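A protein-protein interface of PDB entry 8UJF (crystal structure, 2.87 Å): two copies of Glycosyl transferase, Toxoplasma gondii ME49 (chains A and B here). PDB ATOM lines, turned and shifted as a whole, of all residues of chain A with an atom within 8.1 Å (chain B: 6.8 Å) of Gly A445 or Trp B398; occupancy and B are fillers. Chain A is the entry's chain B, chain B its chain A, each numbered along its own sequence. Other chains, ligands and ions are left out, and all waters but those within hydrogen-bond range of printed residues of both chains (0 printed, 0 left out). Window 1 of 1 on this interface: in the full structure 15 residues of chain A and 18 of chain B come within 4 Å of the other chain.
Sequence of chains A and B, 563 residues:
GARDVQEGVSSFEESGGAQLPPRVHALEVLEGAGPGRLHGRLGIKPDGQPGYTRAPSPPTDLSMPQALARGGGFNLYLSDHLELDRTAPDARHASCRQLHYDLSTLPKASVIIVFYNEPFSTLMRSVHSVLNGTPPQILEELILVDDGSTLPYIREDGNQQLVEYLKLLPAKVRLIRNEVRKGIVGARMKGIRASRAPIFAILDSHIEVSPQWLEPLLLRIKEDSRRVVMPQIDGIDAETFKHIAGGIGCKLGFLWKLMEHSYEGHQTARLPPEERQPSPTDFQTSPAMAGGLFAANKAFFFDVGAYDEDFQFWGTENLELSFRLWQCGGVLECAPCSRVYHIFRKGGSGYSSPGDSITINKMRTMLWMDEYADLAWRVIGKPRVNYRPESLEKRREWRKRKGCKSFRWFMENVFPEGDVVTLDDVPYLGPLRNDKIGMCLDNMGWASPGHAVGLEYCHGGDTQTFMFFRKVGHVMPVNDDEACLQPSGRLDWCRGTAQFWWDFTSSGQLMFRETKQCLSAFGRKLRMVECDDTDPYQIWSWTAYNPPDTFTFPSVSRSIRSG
N of Asp A462 sits at hydrogen-bond distance from OD1 of Asp B303, at 3.4 Å. OD1 of Asp B303 lies close to N of Thr A463 (3.5 Å). NE1 of Trp B398 is in hydrogen-bond range of O of Gly A445.
N of Gly A445 is in hydrogen-bond range of OD1 of Asn A443 (2.5 Å). N of Asn A443 sits at hydrogen-bond distance from O of Thr A463. The backbone carbonyl oxygen (O) of Asp A462 sits close to the side-chain amide oxygen (OD1) of Asn A479 (3.3 Å). SG of Cys B404 is disulfide-bonded to SG of Cys B328 (2.0 Å).
CB of Ser A448 touches NH1 of Arg B401, 3.7 Å away. His A451 touches Lys B394 (NE2 to CD, 3.4 Å). O of Phe B302 touches CG2 of Thr A463, 3.5 Å away. Asn A479 touches Arg B401.
Of the printed residues of chain B, His A451 touches Lys B394. Of the printed residues of chain B, Thr A463 touches Phe B302 and Asp B303. Glu B393 touches none of the printed residues of chain A. Trp B398 touches just one residue of chain A: Gly A445. Printed residues of chain A within 4 Å of Arg B401: Ser A448 (3.7 Å) and Asn A479 (3.9 Å). The nearest printed residue of chain B that does not touch Ser A448 is Glu B397 (5.5 Å).
Of the 20 printed residues of chain B, 5 touch a printed residue of chain A. Printed residues of chain B that touch a printed residue of chain A: Phe B302, Asp B303, Lys B394, Trp B398 and Arg B401. Hydrophobic or aromatic side chains of chain B within 4 Å of the printed part of chain A: Trp B398. Hydrophobic or aromatic side chains of chain A that line the printed part of chain B: His A451. Among the printed residues, no Asp or Glu carboxylate lies within 4 Å of a Lys or Arg side-chain nitrogen of the other chain.
No position is printed for both chains.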
ATOM      1  N   ASP A 442     -16.718  18.613   1.623  1.00  0.00           N
ATOM      2  CA  ASP A 442     -16.735  17.564   2.634  1.00  0.00           C
ATOM      3  C   ASP A 442     -15.591  16.600   2.367  1.00  0.00           C
ATOM      4  O   ASP A 442     -15.456  16.094   1.250  1.00  0.00           O
ATOM      5  CB  ASP A 442     -18.081  16.828   2.618  1.00  0.00           C
ATOM      6  CG  ASP A 442     -18.410  16.176   3.944  1.00  0.00           C
ATOM      7  OD1 ASP A 442     -17.519  15.532   4.534  1.00  0.00           O
ATOM      8  OD2 ASP A 442     -19.565  16.320   4.397  1.00  0.00           O
ATOM      9  N   ASN A 443     -14.772  16.353   3.393  1.00  0.00           N
ATOM     10  CA  ASN A 443     -13.705  15.364   3.299  1.00  0.00           C
ATOM     11  C   ASN A 443     -14.225  13.930   3.298  1.00  0.00           C
ATOM     12  O   ASN A 443     -13.445  13.008   3.040  1.00  0.00           O
ATOM     13  CB  ASN A 443     -12.709  15.568   4.450  1.00  0.00           C
ATOM     14  CG  ASN A 443     -13.326  15.322   5.816  1.00  0.00           C
ATOM     15  OD1 ASN A 443     -14.281  14.558   5.955  1.00  0.00           O
ATOM     16  ND2 ASN A 443     -12.788  15.986   6.833  1.00  0.00           N
ATOM     17  N   MET A 444     -15.514  13.725   3.574  1.00  0.00           N
ATOM     18  CA  MET A 444     -16.137  12.402   3.584  1.00  0.00           C
ATOM     19  C   MET A 444     -15.630  11.549   4.745  1.00  0.00           C
ATOM     20  O   MET A 444     -15.655  10.318   4.682  1.00  0.00           O
ATOM     21  CB  MET A 444     -15.908  11.669   2.260  1.00  0.00           C
ATOM     22  CG  MET A 444     -16.219  12.490   1.013  1.00  0.00           C
ATOM     23  SD  MET A 444     -17.742  13.466   1.030  1.00  0.00           S
ATOM     24  CE  MET A 444     -18.907  12.368   1.834  1.00  0.00           C
ATOM     25  N   GLY A 445     -15.178  12.208   5.810  1.00  0.00           N
ATOM     26  CA  GLY A 445     -14.780  11.564   7.041  1.00  0.00           C
ATOM     27  C   GLY A 445     -13.310  11.229   7.155  1.00  0.00           C
ATOM     28  O   GLY A 445     -12.848  10.925   8.264  1.00  0.00           O
ATOM     29  N   TRP A 446     -12.557  11.266   6.057  1.00  0.00           N
ATOM     30  CA  TRP A 446     -11.117  11.008   6.074  1.00  0.00           C
ATOM     31  C   TRP A 446     -10.388  12.275   5.622  1.00  0.00           C
ATOM     32  O   TRP A 446     -10.333  12.574   4.423  1.00  0.00           O
ATOM     33  CB  TRP A 446     -10.752   9.799   5.210  1.00  0.00           C
ATOM     34  CG  TRP A 446     -11.643   9.588   4.032  1.00  0.00           C
ATOM     35  CD1 TRP A 446     -11.555  10.203   2.823  1.00  0.00           C
ATOM     36  CD2 TRP A 446     -12.761   8.693   3.947  1.00  0.00           C
ATOM     37  NE1 TRP A 446     -12.547   9.752   1.987  1.00  0.00           N
ATOM     38  CE2 TRP A 446     -13.301   8.825   2.653  1.00  0.00           C
ATOM     39  CE3 TRP A 446     -13.356   7.794   4.840  1.00  0.00           C
ATOM     40  CZ2 TRP A 446     -14.411   8.093   2.229  1.00  0.00           C
ATOM     41  CZ3 TRP A 446     -14.459   7.070   4.417  1.00  0.00           C
ATOM     42  CH2 TRP A 446     -14.973   7.224   3.123  1.00  0.00           C
ATOM     43  N   ALA A 447      -9.839  13.024   6.581  1.00  0.00           N
ATOM     44  CA  ALA A 447      -9.049  14.210   6.276  1.00  0.00           C
ATOM     45  C   ALA A 447      -7.659  13.856   5.768  1.00  0.00           C
ATOM     46  O   ALA A 447      -6.934  14.744   5.307  1.00  0.00           O
ATOM     47  CB  ALA A 447      -8.922  15.107   7.512  1.00  0.00           C
ATOM     48  N   SER A 448      -7.278  12.586   5.841  1.00  0.00           N
ATOM     49  CA  SER A 448      -5.965  12.177   5.369  1.00  0.00           C
ATOM     50  C   SER A 448      -5.858  12.413   3.863  1.00  0.00           C
ATOM     51  O   SER A 448      -6.835  12.209   3.125  1.00  0.00           O
ATOM     52  CB  SER A 448      -5.735  10.699   5.699  1.00  0.00           C
ATOM     53  OG  SER A 448      -6.703   9.860   5.083  1.00  0.00           O
ATOM     54  N   HIS A 451      -7.911  11.082  -0.797  1.00  0.00           N
ATOM     55  CA  HIS A 451      -9.286  10.790  -1.187  1.00  0.00           C
ATOM     56  C   HIS A 451      -9.987  12.027  -1.753  1.00  0.00           C
ATOM     57  O   HIS A 451      -9.488  13.152  -1.681  1.00  0.00           O
ATOM     58  CB  HIS A 451     -10.063  10.190  -0.009  1.00  0.00           C
ATOM     59  CG  HIS A 451      -9.352   9.050   0.658  1.00  0.00           C
ATOM     60  ND1 HIS A 451      -8.358   9.236   1.595  1.00  0.00           N
ATOM     61  CD2 HIS A 451      -9.490   7.709   0.519  1.00  0.00           C
ATOM     62  CE1 HIS A 451      -7.917   8.059   2.007  1.00  0.00           C
ATOM     63  NE2 HIS A 451      -8.586   7.116   1.369  1.00  0.00           N
ATOM     64  N   ALA A 452     -11.151  11.790  -2.362  1.00  0.00           N
ATOM     65  CA  ALA A 452     -11.863  12.815  -3.106  1.00  0.00           C
ATOM     66  C   ALA A 452     -12.790  13.618  -2.201  1.00  0.00           C
ATOM     67  O   ALA A 452     -13.311  13.113  -1.202  1.00  0.00           O
ATOM     68  CB  ALA A 452     -12.684  12.191  -4.238  1.00  0.00           C
ATOM     69  N   ASP A 462     -16.650  19.583  11.848  1.00  0.00           N
ATOM     70  CA  ASP A 462     -15.240  19.639  11.480  1.00  0.00           C
ATOM     71  C   ASP A 462     -14.996  18.962  10.140  1.00  0.00           C
ATOM     72  O   ASP A 462     -14.043  19.308   9.434  1.00  0.00           O
ATOM     73  CB  ASP A 462     -14.384  18.990  12.570  1.00  0.00           C
ATOM     74  CG  ASP A 462     -14.306  19.829  13.837  1.00  0.00           C
ATOM     75  OD1 ASP A 462     -14.125  21.062  13.734  1.00  0.00           O
ATOM     76  OD2 ASP A 462     -14.423  19.252  14.939  1.00  0.00           O
ATOM     77  N   THR A 463     -15.838  17.994   9.774  1.00  0.00           N
ATOM     78  CA  THR A 463     -15.685  17.331   8.487  1.00  0.00           C
ATOM     79  C   THR A 463     -15.940  18.278   7.323  1.00  0.00           C
ATOM     80  O   THR A 463     -15.530  17.981   6.195  1.00  0.00           O
ATOM     81  CB  THR A 463     -16.649  16.149   8.391  1.00  0.00           C
ATOM     82  OG1 THR A 463     -17.984  16.598   8.667  1.00  0.00           O
ATOM     83  CG2 THR A 463     -16.274  15.076   9.405  1.00  0.00           C
ATOM     84  N   GLN A 464     -16.599  19.411   7.576  1.00  0.00           N
ATOM     85  CA  GLN A 464     -16.918  20.392   6.546  1.00  0.00           C
ATOM     86  C   GLN A 464     -16.227  21.729   6.785  1.00  0.00           C
ATOM     87  O   GLN A 464     -16.719  22.765   6.328  1.00  0.00           O
ATOM     88  CB  GLN A 464     -18.432  20.581   6.455  1.00  0.00           C
ATOM     89  CG  GLN A 464     -19.157  19.362   5.911  1.00  0.00           C
ATOM     90  CD  GLN A 464     -20.660  19.483   6.020  1.00  0.00           C
ATOM     91  OE1 GLN A 464     -21.173  20.352   6.725  1.00  0.00           O
ATOM     92  NE2 GLN A 464     -21.374  18.609   5.323  1.00  0.00           N
ATOM     93  N   ASN A 479      -8.604  19.591  10.027  1.00  0.00           N
ATOM     94  CA  ASN A 479      -8.041  18.512  10.824  1.00  0.00           C
ATOM     95  C   ASN A 479      -6.767  17.927  10.229  1.00  0.00           C
ATOM     96  O   ASN A 479      -6.312  16.878  10.697  1.00  0.00           O
ATOM     97  CB  ASN A 479      -9.097  17.425  10.987  1.00  0.00           C
ATOM     98  CG  ASN A 479     -10.369  17.958  11.608  1.00  0.00           C
ATOM     99  OD1 ASN A 479     -11.148  18.633  10.934  1.00  0.00           O
ATOM    100  ND2 ASN A 479     -10.567  17.706  12.895  1.00  0.00           N
ATOM    101  N   PHE B 302     -21.186  12.843  12.548  1.00  0.00           N
ATOM    102  CA  PHE B 302     -20.186  12.764  11.488  1.00  0.00           C
ATOM    103  C   PHE B 302     -18.769  12.977  12.003  1.00  0.00           C
ATOM    104  O   PHE B 302     -17.814  12.554  11.346  1.00  0.00           O
ATOM    105  CB  PHE B 302     -20.501  13.778  10.387  1.00  0.00           C
ATOM    106  CG  PHE B 302     -21.586  13.329   9.448  1.00  0.00           C
ATOM    107  CD1 PHE B 302     -21.351  12.326   8.524  1.00  0.00           C
ATOM    108  CD2 PHE B 302     -22.838  13.920   9.477  1.00  0.00           C
ATOM    109  CE1 PHE B 302     -22.350  11.910   7.656  1.00  0.00           C
ATOM    110  CE2 PHE B 302     -23.839  13.511   8.608  1.00  0.00           C
ATOM    111  CZ  PHE B 302     -23.594  12.505   7.698  1.00  0.00           C
ATOM    112  N   ASP B 303     -18.610  13.607  13.159  1.00  0.00           N
ATOM    113  CA  ASP B 303     -17.289  13.813  13.730  1.00  0.00           C
ATOM    114  C   ASP B 303     -16.836  12.635  14.579  1.00  0.00           C
ATOM    115  O   ASP B 303     -15.635  12.502  14.840  1.00  0.00           O
ATOM    116  CB  ASP B 303     -17.273  15.090  14.577  1.00  0.00           C
ATOM    117  CG  ASP B 303     -17.371  16.351  13.734  1.00  0.00           C
ATOM    118  OD1 ASP B 303     -17.110  16.288  12.512  1.00  0.00           O
ATOM    119  OD2 ASP B 303     -17.719  17.413  14.296  1.00  0.00           O
ATOM    120  N   VAL B 304     -17.767  11.782  15.005  1.00  0.00           N
ATOM    121  CA  VAL B 304     -17.454  10.618  15.828  1.00  0.00           C
ATOM    122  C   VAL B 304     -17.207   9.402  14.938  1.00  0.00           C
ATOM    123  O   VAL B 304     -17.182   8.267  15.419  1.00  0.00           O
ATOM    124  CB  VAL B 304     -18.573  10.341  16.852  1.00  0.00           C
ATOM    125  CG1 VAL B 304     -18.135   9.283  17.856  1.00  0.00           C
ATOM    126  CG2 VAL B 304     -18.969  11.616  17.586  1.00  0.00           C
ATOM    127  N   GLY B 305     -17.020   9.636  13.632  1.00  0.00           N
ATOM    128  CA  GLY B 305     -16.816   8.582  12.655  1.00  0.00           C
ATOM    129  C   GLY B 305     -18.043   8.162  11.869  1.00  0.00           C
ATOM    130  O   GLY B 305     -17.895   7.632  10.761  1.00  0.00           O
ATOM    131  N   ALA B 306     -19.241   8.364  12.395  1.00  0.00           N
ATOM    132  CA  ALA B 306     -20.431   8.019  11.646  1.00  0.00           C
ATOM    133  C   ALA B 306     -20.695   6.527  11.609  1.00  0.00           C
ATOM    134  O   ALA B 306     -21.163   5.953  12.596  1.00  0.00           O
ATOM    135  N   ARG B 324     -16.733   2.664  19.284  1.00  0.00           N
ATOM    136  CA  ARG B 324     -16.138   3.891  18.762  1.00  0.00           C
ATOM    137  C   ARG B 324     -16.741   5.121  19.429  1.00  0.00           C
ATOM    138  O   ARG B 324     -16.021   6.065  19.778  1.00  0.00           O
ATOM    139  CB  ARG B 324     -16.307   3.950  17.241  1.00  0.00           C
ATOM    140  CG  ARG B 324     -16.075   5.327  16.643  1.00  0.00           C
ATOM    141  CD  ARG B 324     -15.877   5.278  15.129  1.00  0.00           C
ATOM    142  NE  ARG B 324     -16.760   4.343  14.441  1.00  0.00           N
ATOM    143  CZ  ARG B 324     -17.994   4.621  14.043  1.00  0.00           C
ATOM    144  NH1 ARG B 324     -18.552   5.795  14.290  1.00  0.00           N
ATOM    145  NH2 ARG B 324     -18.684   3.699  13.379  1.00  0.00           N
ATOM    146  N   CYS B 328     -14.357   7.737  21.617  1.00  0.00           N
ATOM    147  CA  CYS B 328     -14.039   8.978  20.921  1.00  0.00           C
ATOM    148  C   CYS B 328     -14.824  10.168  21.473  1.00  0.00           C
ATOM    149  O   CYS B 328     -15.070  11.143  20.757  1.00  0.00           O
ATOM    150  CB  CYS B 328     -14.287   8.821  19.423  1.00  0.00           C
ATOM    151  SG  CYS B 328     -13.493   7.359  18.709  1.00  0.00           S
ATOM    152  N   TRP B 368     -11.468  -1.923  17.231  1.00  0.00           N
ATOM    153  CA  TRP B 368     -11.742  -1.080  18.383  1.00  0.00           C
ATOM    154  C   TRP B 368     -11.618  -1.825  19.701  1.00  0.00           C
ATOM    155  O   TRP B 368     -11.862  -1.230  20.755  1.00  0.00           O
ATOM    156  CB  TRP B 368     -13.138  -0.468  18.235  1.00  0.00           C
ATOM    157  CG  TRP B 368     -13.251   0.264  16.937  1.00  0.00           C
ATOM    158  CD1 TRP B 368     -13.594  -0.263  15.728  1.00  0.00           C
ATOM    159  CD2 TRP B 368     -12.983   1.648  16.711  1.00  0.00           C
ATOM    160  NE1 TRP B 368     -13.564   0.711  14.762  1.00  0.00           N
ATOM    161  CE2 TRP B 368     -13.193   1.895  15.342  1.00  0.00           C
ATOM    162  CE3 TRP B 368     -12.588   2.705  17.534  1.00  0.00           C
ATOM    163  CZ2 TRP B 368     -13.026   3.151  14.779  1.00  0.00           C
ATOM    164  CZ3 TRP B 368     -12.427   3.951  16.974  1.00  0.00           C
ATOM    165  CH2 TRP B 368     -12.638   4.163  15.610  1.00  0.00           C
ATOM    166  N   GLU B 393      -7.238   0.196   7.689  1.00  0.00           N
ATOM    167  CA  GLU B 393      -6.104   0.951   8.207  1.00  0.00           C
ATOM    168  C   GLU B 393      -6.432   2.438   8.290  1.00  0.00           C
ATOM    169  O   GLU B 393      -5.961   3.127   9.201  1.00  0.00           O
ATOM    170  CB  GLU B 393      -4.879   0.715   7.323  1.00  0.00           C
ATOM    171  CG  GLU B 393      -3.578   1.326   7.839  1.00  0.00           C
ATOM    172  CD  GLU B 393      -3.017   0.570   9.037  1.00  0.00           C
ATOM    173  OE1 GLU B 393      -2.937  -0.678   8.973  1.00  0.00           O
ATOM    174  OE2 GLU B 393      -2.658   1.216  10.042  1.00  0.00           O
ATOM    175  N   LYS B 394      -7.245   2.944   7.355  1.00  0.00           N
ATOM    176  CA  LYS B 394      -7.654   4.343   7.402  1.00  0.00           C
ATOM    177  C   LYS B 394      -8.469   4.638   8.653  1.00  0.00           C
ATOM    178  O   LYS B 394      -8.479   5.774   9.139  1.00  0.00           O
ATOM    179  CB  LYS B 394      -8.489   4.675   6.166  1.00  0.00           C
ATOM    180  CG  LYS B 394      -7.782   4.466   4.841  1.00  0.00           C
ATOM    181  CD  LYS B 394      -8.755   4.679   3.688  1.00  0.00           C
ATOM    182  CE  LYS B 394      -8.315   3.928   2.435  1.00  0.00           C
ATOM    183  NZ  LYS B 394      -9.486   3.318   1.726  1.00  0.00           N
ATOM    184  N   ARG B 395      -9.149   3.623   9.189  1.00  0.00           N
ATOM    185  CA  ARG B 395      -9.782   3.746  10.497  1.00  0.00           C
ATOM    186  C   ARG B 395      -8.752   3.698  11.616  1.00  0.00           C
ATOM    187  O   ARG B 395      -8.875   4.418  12.613  1.00  0.00           O
ATOM    188  CB  ARG B 395     -10.813   2.631  10.672  1.00  0.00           C
ATOM    189  CG  ARG B 395     -12.109   2.822   9.906  1.00  0.00           C
ATOM    190  CD  ARG B 395     -13.063   3.662  10.754  1.00  0.00           C
ATOM    191  NE  ARG B 395     -14.047   4.416   9.989  1.00  0.00           N
ATOM    192  CZ  ARG B 395     -15.210   4.830  10.475  1.00  0.00           C
ATOM    193  NH1 ARG B 395     -15.590   4.537  11.708  1.00  0.00           N
ATOM    194  NH2 ARG B 395     -16.010   5.565   9.706  1.00  0.00           N
ATOM    195  N   ARG B 396      -7.728   2.859  11.464  1.00  0.00           N
ATOM    196  CA  ARG B 396      -6.670   2.789  12.466  1.00  0.00           C
ATOM    197  C   ARG B 396      -5.946   4.127  12.577  1.00  0.00           C
ATOM    198  O   ARG B 396      -5.637   4.581  13.686  1.00  0.00           O
ATOM    199  CB  ARG B 396      -5.734   1.634  12.100  1.00  0.00           C
ATOM    200  CG  ARG B 396      -4.998   0.967  13.258  1.00  0.00           C
ATOM    201  CD  ARG B 396      -4.439  -0.375  12.779  1.00  0.00           C
ATOM    202  NE  ARG B 396      -3.533  -1.029  13.717  1.00  0.00           N
ATOM    203  CZ  ARG B 396      -3.799  -2.138  14.399  1.00  0.00           C
ATOM    204  NH1 ARG B 396      -4.963  -2.761  14.290  1.00  0.00           N
ATOM    205  NH2 ARG B 396      -2.862  -2.650  15.192  1.00  0.00           N
ATOM    206  N   GLU B 397      -5.686   4.784  11.444  1.00  0.00           N
ATOM    207  CA  GLU B 397      -5.179   6.155  11.483  1.00  0.00           C
ATOM    208  C   GLU B 397      -6.241   7.135  11.970  1.00  0.00           C
ATOM    209  O   GLU B 397      -5.968   7.983  12.828  1.00  0.00           O
ATOM    210  CB  GLU B 397      -4.634   6.577  10.111  1.00  0.00           C
ATOM    211  CG  GLU B 397      -3.227   6.043   9.822  1.00  0.00           C
ATOM    212  CD  GLU B 397      -3.002   5.589   8.388  1.00  0.00           C
ATOM    213  OE1 GLU B 397      -3.828   5.909   7.507  1.00  0.00           O
ATOM    214  OE2 GLU B 397      -1.989   4.897   8.144  1.00  0.00           O
ATOM    215  N   TRP B 398      -7.462   7.037  11.441  1.00  0.00           N
ATOM    216  CA  TRP B 398      -8.523   7.924  11.907  1.00  0.00           C
ATOM    217  C   TRP B 398      -8.682   7.831  13.418  1.00  0.00           C
ATOM    218  O   TRP B 398      -8.838   8.851  14.100  1.00  0.00           O
ATOM    219  CB  TRP B 398      -9.846   7.583  11.219  1.00  0.00           C
ATOM    220  CG  TRP B 398     -10.941   8.558  11.532  1.00  0.00           C
ATOM    221  CD1 TRP B 398     -11.327   9.616  10.765  1.00  0.00           C
ATOM    222  CD2 TRP B 398     -11.790   8.574  12.691  1.00  0.00           C
ATOM    223  NE1 TRP B 398     -12.359  10.291  11.368  1.00  0.00           N
ATOM    224  CE2 TRP B 398     -12.662   9.673  12.552  1.00  0.00           C
ATOM    225  CE3 TRP B 398     -11.896   7.769  13.830  1.00  0.00           C
ATOM    226  CZ2 TRP B 398     -13.629   9.988  13.508  1.00  0.00           C
ATOM    227  CZ3 TRP B 398     -12.860   8.083  14.782  1.00  0.00           C
ATOM    228  CH2 TRP B 398     -13.712   9.182  14.613  1.00  0.00           C
ATOM    229  N   ARG B 399      -8.635   6.611  13.959  1.00  0.00           N
ATOM    230  CA  ARG B 399      -8.798   6.438  15.398  1.00  0.00           C
ATOM    231  C   ARG B 399      -7.678   7.130  16.159  1.00  0.00           C
ATOM    232  O   ARG B 399      -7.901   7.690  17.240  1.00  0.00           O
ATOM    233  CB  ARG B 399      -8.830   4.952  15.754  1.00  0.00           C
ATOM    234  CG  ARG B 399      -9.146   4.679  17.218  1.00  0.00           C
ATOM    235  CD  ARG B 399      -8.981   3.204  17.548  1.00  0.00           C
ATOM    236  NE  ARG B 399      -9.302   2.910  18.940  1.00  0.00           N
ATOM    237  CZ  ARG B 399      -8.889   1.836  19.599  1.00  0.00           C
ATOM    238  NH1 ARG B 399      -8.101   0.936  19.033  1.00  0.00           N
ATOM    239  NH2 ARG B 399      -9.275   1.660  20.860  1.00  0.00           N
ATOM    240  N   LYS B 400      -6.460   7.089  15.617  1.00  0.00           N
ATOM    241  CA  LYS B 400      -5.318   7.647  16.328  1.00  0.00           C
ATOM    242  C   LYS B 400      -5.243   9.157  16.139  1.00  0.00           C
ATOM    243  O   LYS B 400      -4.777   9.866  17.036  1.00  0.00           O
ATOM    244  CB  LYS B 400      -4.034   6.973  15.846  1.00  0.00           C
ATOM    245  CG  LYS B 400      -2.988   6.722  16.937  1.00  0.00           C
ATOM    246  CD  LYS B 400      -3.545   5.760  18.008  1.00  0.00           C
ATOM    247  CE  LYS B 400      -2.611   5.572  19.198  1.00  0.00           C
ATOM    248  NZ  LYS B 400      -3.278   4.782  20.279  1.00  0.00           N
ATOM    249  N   ARG B 401      -5.693   9.661  14.983  1.00  0.00           N
ATOM    250  CA  ARG B 401      -5.771  11.102  14.767  1.00  0.00           C
ATOM    251  C   ARG B 401      -6.849  11.755  15.627  1.00  0.00           C
ATOM    252  O   ARG B 401      -6.769  12.958  15.893  1.00  0.00           O
ATOM    253  CB  ARG B 401      -6.035  11.390  13.283  1.00  0.00           C
ATOM    254  CG  ARG B 401      -5.823  12.841  12.864  1.00  0.00           C
ATOM    255  CD  ARG B 401      -6.060  13.053  11.360  1.00  0.00           C
ATOM    256  NE  ARG B 401      -4.916  12.654  10.544  1.00  0.00           N
ATOM    257  CZ  ARG B 401      -4.922  11.690   9.629  1.00  0.00           C
ATOM    258  NH1 ARG B 401      -6.021  11.010   9.342  1.00  0.00           N
ATOM    259  NH2 ARG B 401      -3.797  11.408   8.979  1.00  0.00           N
ATOM    260  N   LYS B 402      -7.843  10.990  16.074  1.00  0.00           N
ATOM    261  CA  LYS B 402      -8.892  11.493  16.950  1.00  0.00           C
ATOM    262  C   LYS B 402      -8.552  11.348  18.426  1.00  0.00           C
ATOM    263  O   LYS B 402      -9.225  11.959  19.264  1.00  0.00           O
ATOM    264  CB  LYS B 402     -10.209  10.764  16.658  1.00  0.00           C
ATOM    265  CG  LYS B 402     -11.451  11.398  17.277  1.00  0.00           C
ATOM    266  CD  LYS B 402     -11.957  12.597  16.492  1.00  0.00           C
ATOM    267  CE  LYS B 402     -12.898  13.443  17.341  1.00  0.00           C
ATOM    268  NZ  LYS B 402     -13.886  12.596  18.067  1.00  0.00           N
ATOM    269  N   GLY B 403      -7.533  10.565  18.765  1.00  0.00           N
ATOM    270  CA  GLY B 403      -7.205  10.353  20.158  1.00  0.00           C
ATOM    271  C   GLY B 403      -8.229   9.532  20.902  1.00  0.00           C
ATOM    272  O   GLY B 403      -8.398   9.712  22.113  1.00  0.00           O
ATOM    273  N   CYS B 404      -8.939   8.647  20.207  1.00  0.00           N
ATOM    274  CA  CYS B 404      -9.922   7.798  20.868  1.00  0.00           C
ATOM    275  C   CYS B 404      -9.228   6.942  21.922  1.00  0.00           C
ATOM    276  O   CYS B 404      -8.070   6.543  21.773  1.00  0.00           O
ATOM    277  CB  CYS B 404     -10.649   6.921  19.847  1.00  0.00           C
ATOM    278  SG  CYS B 404     -11.523   7.838  18.527  1.00  0.00           S
